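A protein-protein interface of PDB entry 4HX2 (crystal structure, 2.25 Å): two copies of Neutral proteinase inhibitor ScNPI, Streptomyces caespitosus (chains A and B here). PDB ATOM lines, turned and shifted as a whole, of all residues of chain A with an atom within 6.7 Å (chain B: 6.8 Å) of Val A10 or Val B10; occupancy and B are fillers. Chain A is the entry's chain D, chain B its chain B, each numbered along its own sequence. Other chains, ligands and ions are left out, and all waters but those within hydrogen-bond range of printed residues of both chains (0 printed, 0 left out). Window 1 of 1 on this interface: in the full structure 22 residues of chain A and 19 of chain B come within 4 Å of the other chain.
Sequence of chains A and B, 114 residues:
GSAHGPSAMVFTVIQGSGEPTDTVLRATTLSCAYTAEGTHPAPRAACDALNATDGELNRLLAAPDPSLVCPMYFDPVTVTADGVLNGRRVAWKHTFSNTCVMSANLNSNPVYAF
The backbone NH (N) of Met B9 sits at hydrogen-bond distance from the backbone carbonyl oxygen (O) of Leu B30 (2.8 Å). SD of Met B9 sits close to N of Val B84, at 3.8 Å. The backbone NH (N) of Val B10 sits at hydrogen-bond distance from the backbone carbonyl oxygen (O) of Asp B82 (2.9 Å). OG1 of Thr B80 sits at hydrogen-bond distance from OG1 of Thr B12 (2.8 Å). The backbone NH (N) of Val A84 sits at hydrogen-bond distance from the backbone carbonyl oxygen (O) of Ala A8 (2.8 Å). N of Met A9 sits at hydrogen-bond distance from O of Leu A30, 2.8 Å away.
CG2 of Val B10 touches O of Ala A8 (3.5 Å). Thr B29 touches Ala A8. Met A9 touches Thr B29. Val B84 touches Thr A12 (CG2 to CG2, 3.7 Å). CB of Ala A27 touches CB of Ala B8 (3.8 Å). Thr A29 touches Leu B30. Val B10 touches Asp A82 (CG1 to O, 3.4 Å). CB of Asp A82 touches CB of Asp B82, at 3.98 Å. CG1 of Val B10 touches CA of Gly A83, at 3.7 Å. CG2 of Val A84 touches CB of Ala B27 (3.6 Å).
Printed residues of chain B within 4 Å of Val A10: Ala B8, Val B10, Asp B82 and Gly B83. Val B10 touches four residues of chain A. Of the printed residues of chain A, Val B84 touches Thr A12 (3.7 Å) and Ala A27 (3.9 Å). Of the printed residues of chain B, Ala A27 touches Ala B8 (3.8 Å) and Val B84 (3.9 Å). Printed residues of chain A within 4 Å of Asp B82: Val A10 (3.5 Å) and Asp A82 (3.98 Å). Of the printed residues of chain A, Thr B29 touches Ala A8, Met A9, Thr A29 and Leu A30. Phe B114 touches none of the printed residues of chain A. The nearest residue of chain B that does not touch Val A10 is Met B9 (4.6 Å).
Printed residues of chain B that touch a printed residue of chain A: Ala B8, Val B10, Thr B12, Ala B27, Thr B29, Leu B30, Asp B82, Gly B83 and Val B84. Along chain B the printed residues that touch a printed residue of chain A span positions 8 to 84. Of the 16 printed residues of chain A, 10 touch a printed residue of chain B. Printed residues of chain A that touch a printed residue of chain B: Ala A8, Met A9, Val A10, Thr A12, Ala A27, Thr A29, Leu A30, Asp A82, Gly A83 and Val A84. Among the printed residues, no Asp or Glu carboxylate lies within 4 Å of a Lys or Arg side-chain nitrogen of the other chain.
Ala A8 touches Thr B29, but with the chains exchanged Thr A29 does not touch Ala B8 (4.2 Å). Met A9 touches Thr B29, but with the chains exchanged Thr A29 does not touch Met B9 (4.1 Å). Thr A12 touches Val B84, and with the chains exchanged Val A84 touches Thr B12. Asp A82 touches its own counterpart, Asp B82. Positions printed for both chains: 8, 9, 10, 11, 12, 27, 28, 29, 30, 80, 81, 82, 83, 84, 112 and 114. Of the 19 pairs that touch across the chains among the printed residues, 17 have their exchanged pair printed and touching as well.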
ATOM      1  N   ALA A   8       5.462   2.852  -4.746  1.00  0.00           N
ATOM      2  CA  ALA A   8       6.159   1.625  -5.157  1.00  0.00           C
ATOM      3  C   ALA A   8       5.455   1.170  -6.417  1.00  0.00           C
ATOM      4  O   ALA A   8       4.314   0.707  -6.362  1.00  0.00           O
ATOM      5  CB  ALA A   8       6.100   0.572  -4.045  1.00  0.00           C
ATOM      6  N   MET A   9       6.068   1.445  -7.565  1.00  0.00           N
ATOM      7  CA  MET A   9       5.423   1.266  -8.850  1.00  0.00           C
ATOM      8  C   MET A   9       6.211   0.433  -9.849  1.00  0.00           C
ATOM      9  O   MET A   9       7.446   0.382  -9.804  1.00  0.00           O
ATOM     10  CB  MET A   9       5.200   2.649  -9.483  1.00  0.00           C
ATOM     11  CG  MET A   9       4.346   3.631  -8.652  1.00  0.00           C
ATOM     12  SD  MET A   9       2.566   3.305  -8.763  1.00  0.00           S
ATOM     13  CE  MET A   9       2.232   3.827 -10.419  1.00  0.00           C
ATOM     14  N   VAL A  10       5.474  -0.166 -10.803  1.00  0.00           N
ATOM     15  CA  VAL A  10       6.016  -0.871 -11.966  1.00  0.00           C
ATOM     16  C   VAL A  10       5.348  -0.234 -13.180  1.00  0.00           C
ATOM     17  O   VAL A  10       4.117  -0.141 -13.244  1.00  0.00           O
ATOM     18  CB  VAL A  10       5.951  -2.436 -11.945  1.00  0.00           C
ATOM     19  CG1 VAL A  10       4.580  -2.934 -11.560  1.00  0.00           C
ATOM     20  CG2 VAL A  10       6.369  -3.033 -13.292  1.00  0.00           C
ATOM     21  N   PHE A  11       6.175   0.256 -14.114  1.00  0.00           N
ATOM     22  CA  PHE A  11       5.747   0.871 -15.356  1.00  0.00           C
ATOM     23  C   PHE A  11       6.143  -0.039 -16.470  1.00  0.00           C
ATOM     24  O   PHE A  11       7.240  -0.587 -16.423  1.00  0.00           O
ATOM     25  CB  PHE A  11       6.376   2.268 -15.528  1.00  0.00           C
ATOM     26  CG  PHE A  11       6.041   3.214 -14.391  1.00  0.00           C
ATOM     27  CD1 PHE A  11       4.810   3.877 -14.348  1.00  0.00           C
ATOM     28  CD2 PHE A  11       6.951   3.446 -13.368  1.00  0.00           C
ATOM     29  CE1 PHE A  11       4.488   4.729 -13.286  1.00  0.00           C
ATOM     30  CE2 PHE A  11       6.631   4.318 -12.313  1.00  0.00           C
ATOM     31  CZ  PHE A  11       5.402   4.959 -12.285  1.00  0.00           C
ATOM     32  N   THR A  12       5.236  -0.286 -17.431  1.00  0.00           N
ATOM     33  CA  THR A  12       5.551  -1.137 -18.576  1.00  0.00           C
ATOM     34  C   THR A  12       5.060  -0.465 -19.864  1.00  0.00           C
ATOM     35  O   THR A  12       4.245   0.465 -19.825  1.00  0.00           O
ATOM     36  CB  THR A  12       5.008  -2.607 -18.456  1.00  0.00           C
ATOM     37  OG1 THR A  12       3.694  -2.731 -19.003  1.00  0.00           O
ATOM     38  CG2 THR A  12       5.068  -3.189 -17.040  1.00  0.00           C
ATOM     39  N   ALA A  27       9.931  -2.678 -19.189  1.00  0.00           N
ATOM     40  CA  ALA A  27       9.403  -2.487 -17.864  1.00  0.00           C
ATOM     41  C   ALA A  27      10.451  -1.934 -16.952  1.00  0.00           C
ATOM     42  O   ALA A  27      11.635  -2.221 -17.115  1.00  0.00           O
ATOM     43  CB  ALA A  27       8.880  -3.803 -17.310  1.00  0.00           C
ATOM     44  N   THR A  28      10.013  -1.165 -15.963  1.00  0.00           N
ATOM     45  CA  THR A  28      10.913  -0.641 -14.950  1.00  0.00           C
ATOM     46  C   THR A  28      10.179  -0.609 -13.585  1.00  0.00           C
ATOM     47  O   THR A  28       8.952  -0.765 -13.539  1.00  0.00           O
ATOM     48  CB  THR A  28      11.525   0.714 -15.385  1.00  0.00           C
ATOM     49  OG1 THR A  28      12.718   0.902 -14.634  1.00  0.00           O
ATOM     50  CG2 THR A  28      10.585   1.894 -15.199  1.00  0.00           C
ATOM     51  N   THR A  29      10.961  -0.481 -12.491  1.00  0.00           N
ATOM     52  CA  THR A  29      10.466  -0.323 -11.129  1.00  0.00           C
ATOM     53  C   THR A  29      10.898   1.049 -10.619  1.00  0.00           C
ATOM     54  O   THR A  29      11.939   1.584 -11.026  1.00  0.00           O
ATOM     55  CB  THR A  29      10.923  -1.449 -10.189  1.00  0.00           C
ATOM     56  OG1 THR A  29      12.334  -1.384 -10.034  1.00  0.00           O
ATOM     57  CG2 THR A  29      10.487  -2.839 -10.662  1.00  0.00           C
ATOM     58  N   LEU A  30      10.072   1.622  -9.748  1.00  0.00           N
ATOM     59  CA  LEU A  30      10.321   2.908  -9.120  1.00  0.00           C
ATOM     60  C   LEU A  30       9.765   2.929  -7.701  1.00  0.00           C
ATOM     61  O   LEU A  30       8.621   2.556  -7.476  1.00  0.00           O
ATOM     62  CB  LEU A  30       9.695   4.046  -9.950  1.00  0.00           C
ATOM     63  CG  LEU A  30       9.982   5.479  -9.461  1.00  0.00           C
ATOM     64  CD1 LEU A  30      11.423   5.893  -9.743  1.00  0.00           C
ATOM     65  CD2 LEU A  30       9.007   6.445 -10.063  1.00  0.00           C
ATOM     66  N   THR A  80       1.451   1.145 -19.004  1.00  0.00           N
ATOM     67  CA  THR A  80       0.789   0.683 -17.788  1.00  0.00           C
ATOM     68  C   THR A  80       1.539   1.214 -16.567  1.00  0.00           C
ATOM     69  O   THR A  80       2.731   1.490 -16.640  1.00  0.00           O
ATOM     70  CB  THR A  80       0.649  -0.876 -17.719  1.00  0.00           C
ATOM     71  OG1 THR A  80       1.907  -1.436 -17.378  1.00  0.00           O
ATOM     72  CG2 THR A  80       0.110  -1.521 -19.015  1.00  0.00           C
ATOM     73  N   ALA A  81       0.826   1.347 -15.453  1.00  0.00           N
ATOM     74  CA  ALA A  81       1.335   1.779 -14.152  1.00  0.00           C
ATOM     75  C   ALA A  81       0.566   1.029 -13.088  1.00  0.00           C
ATOM     76  O   ALA A  81      -0.655   1.067 -13.084  1.00  0.00           O
ATOM     77  CB  ALA A  81       1.172   3.286 -13.990  1.00  0.00           C
ATOM     78  N   ASP A  82       1.265   0.267 -12.259  1.00  0.00           N
ATOM     79  CA  ASP A  82       0.666  -0.552 -11.201  1.00  0.00           C
ATOM     80  C   ASP A  82       1.483  -0.503  -9.951  1.00  0.00           C
ATOM     81  O   ASP A  82       2.713  -0.548  -9.998  1.00  0.00           O
ATOM     82  CB  ASP A  82       0.517  -2.024 -11.643  1.00  0.00           C
ATOM     83  CG  ASP A  82      -0.397  -2.228 -12.834  1.00  0.00           C
ATOM     84  OD1 ASP A  82      -1.601  -2.504 -12.621  1.00  0.00           O
ATOM     85  OD2 ASP A  82       0.093  -2.138 -13.983  1.00  0.00           O
ATOM     86  N   GLY A  83       0.786  -0.441  -8.834  1.00  0.00           N
ATOM     87  CA  GLY A  83       1.405  -0.451  -7.525  1.00  0.00           C
ATOM     88  C   GLY A  83       0.760   0.498  -6.551  1.00  0.00           C
ATOM     89  O   GLY A  83      -0.463   0.611  -6.493  1.00  0.00           O
ATOM     90  N   VAL A  84       1.593   1.159  -5.761  1.00  0.00           N
ATOM     91  CA  VAL A  84       1.146   2.101  -4.747  1.00  0.00           C
ATOM     92  C   VAL A  84       1.570   3.468  -5.197  1.00  0.00           C
ATOM     93  O   VAL A  84       2.751   3.693  -5.453  1.00  0.00           O
ATOM     94  CB  VAL A  84       1.707   1.743  -3.338  1.00  0.00           C
ATOM     95  CG1 VAL A  84       1.155   2.676  -2.277  1.00  0.00           C
ATOM     96  CG2 VAL A  84       1.376   0.313  -2.965  1.00  0.00           C
ATOM     97  N   TYR A 112       8.120   7.702 -18.226  1.00  0.00           N
ATOM     98  CA  TYR A 112       8.305   6.694 -19.265  1.00  0.00           C
ATOM     99  C   TYR A 112       9.628   6.860 -20.038  1.00  0.00           C
ATOM    100  O   TYR A 112       9.767   6.346 -21.144  1.00  0.00           O
ATOM    101  CB  TYR A 112       7.079   6.618 -20.190  1.00  0.00           C
ATOM    102  CG  TYR A 112       5.924   5.943 -19.486  1.00  0.00           C
ATOM    103  CD1 TYR A 112       5.817   4.556 -19.458  1.00  0.00           C
ATOM    104  CD2 TYR A 112       5.008   6.685 -18.739  1.00  0.00           C
ATOM    105  CE1 TYR A 112       4.814   3.921 -18.716  1.00  0.00           C
ATOM    106  CE2 TYR A 112       3.986   6.063 -18.016  1.00  0.00           C
ATOM    107  CZ  TYR A 112       3.885   4.681 -18.022  1.00  0.00           C
ATOM    108  OH  TYR A 112       2.872   4.069 -17.328  1.00  0.00           O
ATOM    109  N   PHE A 114      12.525   5.241 -19.960  1.00  0.00           N
ATOM    110  CA  PHE A 114      13.220   4.001 -19.588  1.00  0.00           C
ATOM    111  C   PHE A 114      13.291   3.031 -20.788  1.00  0.00           C
ATOM    112  O   PHE A 114      12.564   3.281 -21.776  1.00  0.00           O
ATOM    113  CB  PHE A 114      12.533   3.332 -18.377  1.00  0.00           C
ATOM    114  CG  PHE A 114      11.119   2.827 -18.558  1.00  0.00           C
ATOM    115  CD1 PHE A 114      10.879   1.534 -19.014  1.00  0.00           C
ATOM    116  CD2 PHE A 114      10.035   3.583 -18.125  1.00  0.00           C
ATOM    117  CE1 PHE A 114       9.570   1.037 -19.103  1.00  0.00           C
ATOM    118  CE2 PHE A 114       8.731   3.076 -18.193  1.00  0.00           C
ATOM    119  CZ  PHE A 114       8.506   1.814 -18.698  1.00  0.00           C
ATOM    120  OXT PHE A 114      14.025   2.009 -20.714  1.00  0.00           O
ATOM    121  N   ALA B   8       9.663  -7.687 -13.332  1.00  0.00           N
ATOM    122  CA  ALA B   8       9.596  -6.312 -12.792  1.00  0.00           C
ATOM    123  C   ALA B   8       8.269  -6.264 -12.046  1.00  0.00           C
ATOM    124  O   ALA B   8       7.198  -6.269 -12.663  1.00  0.00           O
ATOM    125  CB  ALA B   8       9.684  -5.278 -13.930  1.00  0.00           C
ATOM    126  N   MET B   9       8.337  -6.387 -10.741  1.00  0.00           N
ATOM    127  CA  MET B   9       7.136  -6.589  -9.924  1.00  0.00           C
ATOM    128  C   MET B   9       6.995  -5.630  -8.737  1.00  0.00           C
ATOM    129  O   MET B   9       7.995  -5.140  -8.205  1.00  0.00           O
ATOM    130  CB  MET B   9       7.168  -8.016  -9.333  1.00  0.00           C
ATOM    131  CG  MET B   9       7.269  -9.158 -10.338  1.00  0.00           C
ATOM    132  SD  MET B   9       5.695  -9.547 -11.084  1.00  0.00           S
ATOM    133  CE  MET B   9       4.823 -10.324  -9.733  1.00  0.00           C
ATOM    134  N   VAL B  10       5.738  -5.429  -8.304  1.00  0.00           N
ATOM    135  CA  VAL B  10       5.365  -4.708  -7.098  1.00  0.00           C
ATOM    136  C   VAL B  10       4.491  -5.670  -6.276  1.00  0.00           C
ATOM    137  O   VAL B  10       3.503  -6.222  -6.770  1.00  0.00           O
ATOM    138  CB  VAL B  10       4.736  -3.286  -7.284  1.00  0.00           C
ATOM    139  CG1 VAL B  10       3.601  -3.302  -8.293  1.00  0.00           C
ATOM    140  CG2 VAL B  10       4.246  -2.719  -5.948  1.00  0.00           C
ATOM    141  N   PHE B  11       4.918  -5.918  -5.031  1.00  0.00           N
ATOM    142  CA  PHE B  11       4.223  -6.764  -4.085  1.00  0.00           C
ATOM    143  C   PHE B  11       3.678  -5.883  -3.002  1.00  0.00           C
ATOM    144  O   PHE B  11       4.372  -4.958  -2.581  1.00  0.00           O
ATOM    145  CB  PHE B  11       5.168  -7.834  -3.521  1.00  0.00           C
ATOM    146  CG  PHE B  11       5.784  -8.723  -4.579  1.00  0.00           C
ATOM    147  CD1 PHE B  11       5.070  -9.787  -5.118  1.00  0.00           C
ATOM    148  CD2 PHE B  11       7.084  -8.499  -5.029  1.00  0.00           C
ATOM    149  CE1 PHE B  11       5.633 -10.595  -6.107  1.00  0.00           C
ATOM    150  CE2 PHE B  11       7.648  -9.314  -6.019  1.00  0.00           C
ATOM    151  CZ  PHE B  11       6.919 -10.364  -6.544  1.00  0.00           C
ATOM    152  N   THR B  12       2.404  -6.093  -2.606  1.00  0.00           N
ATOM    153  CA  THR B  12       1.810  -5.309  -1.526  1.00  0.00           C
ATOM    154  C   THR B  12       1.076  -6.243  -0.574  1.00  0.00           C
ATOM    155  O   THR B  12       0.780  -7.389  -0.913  1.00  0.00           O
ATOM    156  CB  THR B  12       0.871  -4.135  -2.013  1.00  0.00           C
ATOM    157  OG1 THR B  12      -0.487  -4.562  -2.164  1.00  0.00           O
ATOM    158  CG2 THR B  12       1.358  -3.427  -3.272  1.00  0.00           C
ATOM    159  N   ALA B  27       4.471  -2.345   0.956  1.00  0.00           N
ATOM    160  CA  ALA B  27       4.737  -2.546  -0.463  1.00  0.00           C
ATOM    161  C   ALA B  27       6.222  -2.562  -0.740  1.00  0.00           C
ATOM    162  O   ALA B  27       6.993  -1.901  -0.036  1.00  0.00           O
ATOM    163  CB  ALA B  27       4.076  -1.468  -1.297  1.00  0.00           C
ATOM    164  N   THR B  28       6.631  -3.277  -1.812  1.00  0.00           N
ATOM    165  CA  THR B  28       8.026  -3.331  -2.236  1.00  0.00           C
ATOM    166  C   THR B  28       8.108  -3.586  -3.733  1.00  0.00           C
ATOM    167  O   THR B  28       7.136  -4.029  -4.359  1.00  0.00           O
ATOM    168  CB  THR B  28       8.846  -4.357  -1.414  1.00  0.00           C
ATOM    169  OG1 THR B  28      10.209  -3.967  -1.503  1.00  0.00           O
ATOM    170  CG2 THR B  28       8.691  -5.783  -1.908  1.00  0.00           C
ATOM    171  N   THR B  29       9.284  -3.295  -4.303  1.00  0.00           N
ATOM    172  CA  THR B  29       9.559  -3.500  -5.729  1.00  0.00           C
ATOM    173  C   THR B  29      10.661  -4.541  -5.892  1.00  0.00           C
ATOM    174  O   THR B  29      11.526  -4.678  -5.027  1.00  0.00           O
ATOM    175  CB  THR B  29       9.927  -2.182  -6.436  1.00  0.00           C
ATOM    176  OG1 THR B  29      11.148  -1.690  -5.894  1.00  0.00           O
ATOM    177  CG2 THR B  29       8.831  -1.122  -6.331  1.00  0.00           C
ATOM    178  N   LEU B  30      10.614  -5.277  -7.001  1.00  0.00           N
ATOM    179  CA  LEU B  30      11.583  -6.315  -7.318  1.00  0.00           C
ATOM    180  C   LEU B  30      11.813  -6.375  -8.827  1.00  0.00           C
ATOM    181  O   LEU B  30      10.855  -6.378  -9.590  1.00  0.00           O
ATOM    182  CB  LEU B  30      11.112  -7.691  -6.782  1.00  0.00           C
ATOM    183  CG  LEU B  30      12.064  -8.871  -6.993  1.00  0.00           C
ATOM    184  CD1 LEU B  30      13.244  -8.784  -6.054  1.00  0.00           C
ATOM    185  CD2 LEU B  30      11.355 -10.181  -6.819  1.00  0.00           C
ATOM    186  N   THR B  80      -0.828  -8.998  -2.848  1.00  0.00           N
ATOM    187  CA  THR B  80      -0.961  -8.703  -4.280  1.00  0.00           C
ATOM    188  C   THR B  80       0.413  -8.789  -4.945  1.00  0.00           C
ATOM    189  O   THR B  80       1.441  -8.611  -4.288  1.00  0.00           O
ATOM    190  CB  THR B  80      -1.618  -7.319  -4.546  1.00  0.00           C
ATOM    191  OG1 THR B  80      -0.653  -6.299  -4.306  1.00  0.00           O
ATOM    192  CG2 THR B  80      -2.895  -7.068  -3.717  1.00  0.00           C
ATOM    193  N   ALA B  81       0.414  -9.073  -6.250  1.00  0.00           N
ATOM    194  CA  ALA B  81       1.596  -9.140  -7.119  1.00  0.00           C
ATOM    195  C   ALA B  81       1.188  -8.622  -8.474  1.00  0.00           C
ATOM    196  O   ALA B  81       0.215  -9.104  -9.038  1.00  0.00           O
ATOM    197  CB  ALA B  81       2.110 -10.561  -7.199  1.00  0.00           C
ATOM    198  N   ASP B  82       1.843  -7.561  -8.945  1.00  0.00           N
ATOM    199  CA  ASP B  82       1.546  -6.925 -10.235  1.00  0.00           C
ATOM    200  C   ASP B  82       2.801  -6.545 -10.943  1.00  0.00           C
ATOM    201  O   ASP B  82       3.763  -6.072 -10.329  1.00  0.00           O
ATOM    202  CB  ASP B  82       0.657  -5.680 -10.080  1.00  0.00           C
ATOM    203  CG  ASP B  82      -0.699  -5.950  -9.451  1.00  0.00           C
ATOM    204  OD1 ASP B  82      -1.680  -6.126 -10.210  1.00  0.00           O
ATOM    205  OD2 ASP B  82      -0.785  -5.958  -8.190  1.00  0.00           O
ATOM    206  N   GLY B  83       2.768  -6.712 -12.256  1.00  0.00           N
ATOM    207  CA  GLY B  83       3.889  -6.367 -13.119  1.00  0.00           C
ATOM    208  C   GLY B  83       4.181  -7.412 -14.160  1.00  0.00           C
ATOM    209  O   GLY B  83       3.271  -7.962 -14.776  1.00  0.00           O
ATOM    210  N   VAL B  84       5.452  -7.666 -14.373  1.00  0.00           N
ATOM    211  CA  VAL B  84       5.916  -8.616 -15.372  1.00  0.00           C
ATOM    212  C   VAL B  84       6.567  -9.746 -14.638  1.00  0.00           C
ATOM    213  O   VAL B  84       7.490  -9.518 -13.875  1.00  0.00           O
ATOM    214  CB  VAL B  84       6.880  -7.955 -16.403  1.00  0.00           C
ATOM    215  CG1 VAL B  84       7.262  -8.939 -17.496  1.00  0.00           C
ATOM    216  CG2 VAL B  84       6.251  -6.714 -17.023  1.00  0.00           C
ATOM    217  N   TYR B 112       7.337 -12.439   0.191  1.00  0.00           N
ATOM    218  CA  TYR B 112       6.623 -11.542   1.095  1.00  0.00           C
ATOM    219  C   TYR B 112       7.401 -11.256   2.396  1.00  0.00           C
ATOM    220  O   TYR B 112       6.806 -10.815   3.370  1.00  0.00           O
ATOM    221  CB  TYR B 112       5.191 -12.044   1.349  1.00  0.00           C
ATOM    222  CG  TYR B 112       4.336 -11.792   0.119  1.00  0.00           C
ATOM    223  CD1 TYR B 112       3.742 -10.548  -0.099  1.00  0.00           C
ATOM    224  CD2 TYR B 112       4.218 -12.756  -0.887  1.00  0.00           C
ATOM    225  CE1 TYR B 112       3.052 -10.270  -1.281  1.00  0.00           C
ATOM    226  CE2 TYR B 112       3.498 -12.499  -2.057  1.00  0.00           C
ATOM    227  CZ  TYR B 112       2.913 -11.255  -2.249  1.00  0.00           C
ATOM    228  OH  TYR B 112       2.205 -10.983  -3.401  1.00  0.00           O
ATOM    229  N   PHE B 114       9.201  -8.665   3.446  1.00  0.00           N
ATOM    230  CA  PHE B 114       9.466  -7.226   3.284  1.00  0.00           C
ATOM    231  C   PHE B 114       8.626  -6.402   4.289  1.00  0.00           C
ATOM    232  O   PHE B 114       7.696  -6.989   4.879  1.00  0.00           O
ATOM    233  CB  PHE B 114       9.213  -6.774   1.841  1.00  0.00           C
ATOM    234  CG  PHE B 114       7.792  -6.868   1.329  1.00  0.00           C
ATOM    235  CD1 PHE B 114       6.901  -5.819   1.509  1.00  0.00           C
ATOM    236  CD2 PHE B 114       7.396  -7.930   0.527  1.00  0.00           C
ATOM    237  CE1 PHE B 114       5.613  -5.876   0.974  1.00  0.00           C
ATOM    238  CE2 PHE B 114       6.119  -7.968  -0.032  1.00  0.00           C
ATOM    239  CZ  PHE B 114       5.237  -6.940   0.191  1.00  0.00           C
ATOM    240  OXT PHE B 114       8.852  -5.175   4.436  1.00  0.00           O
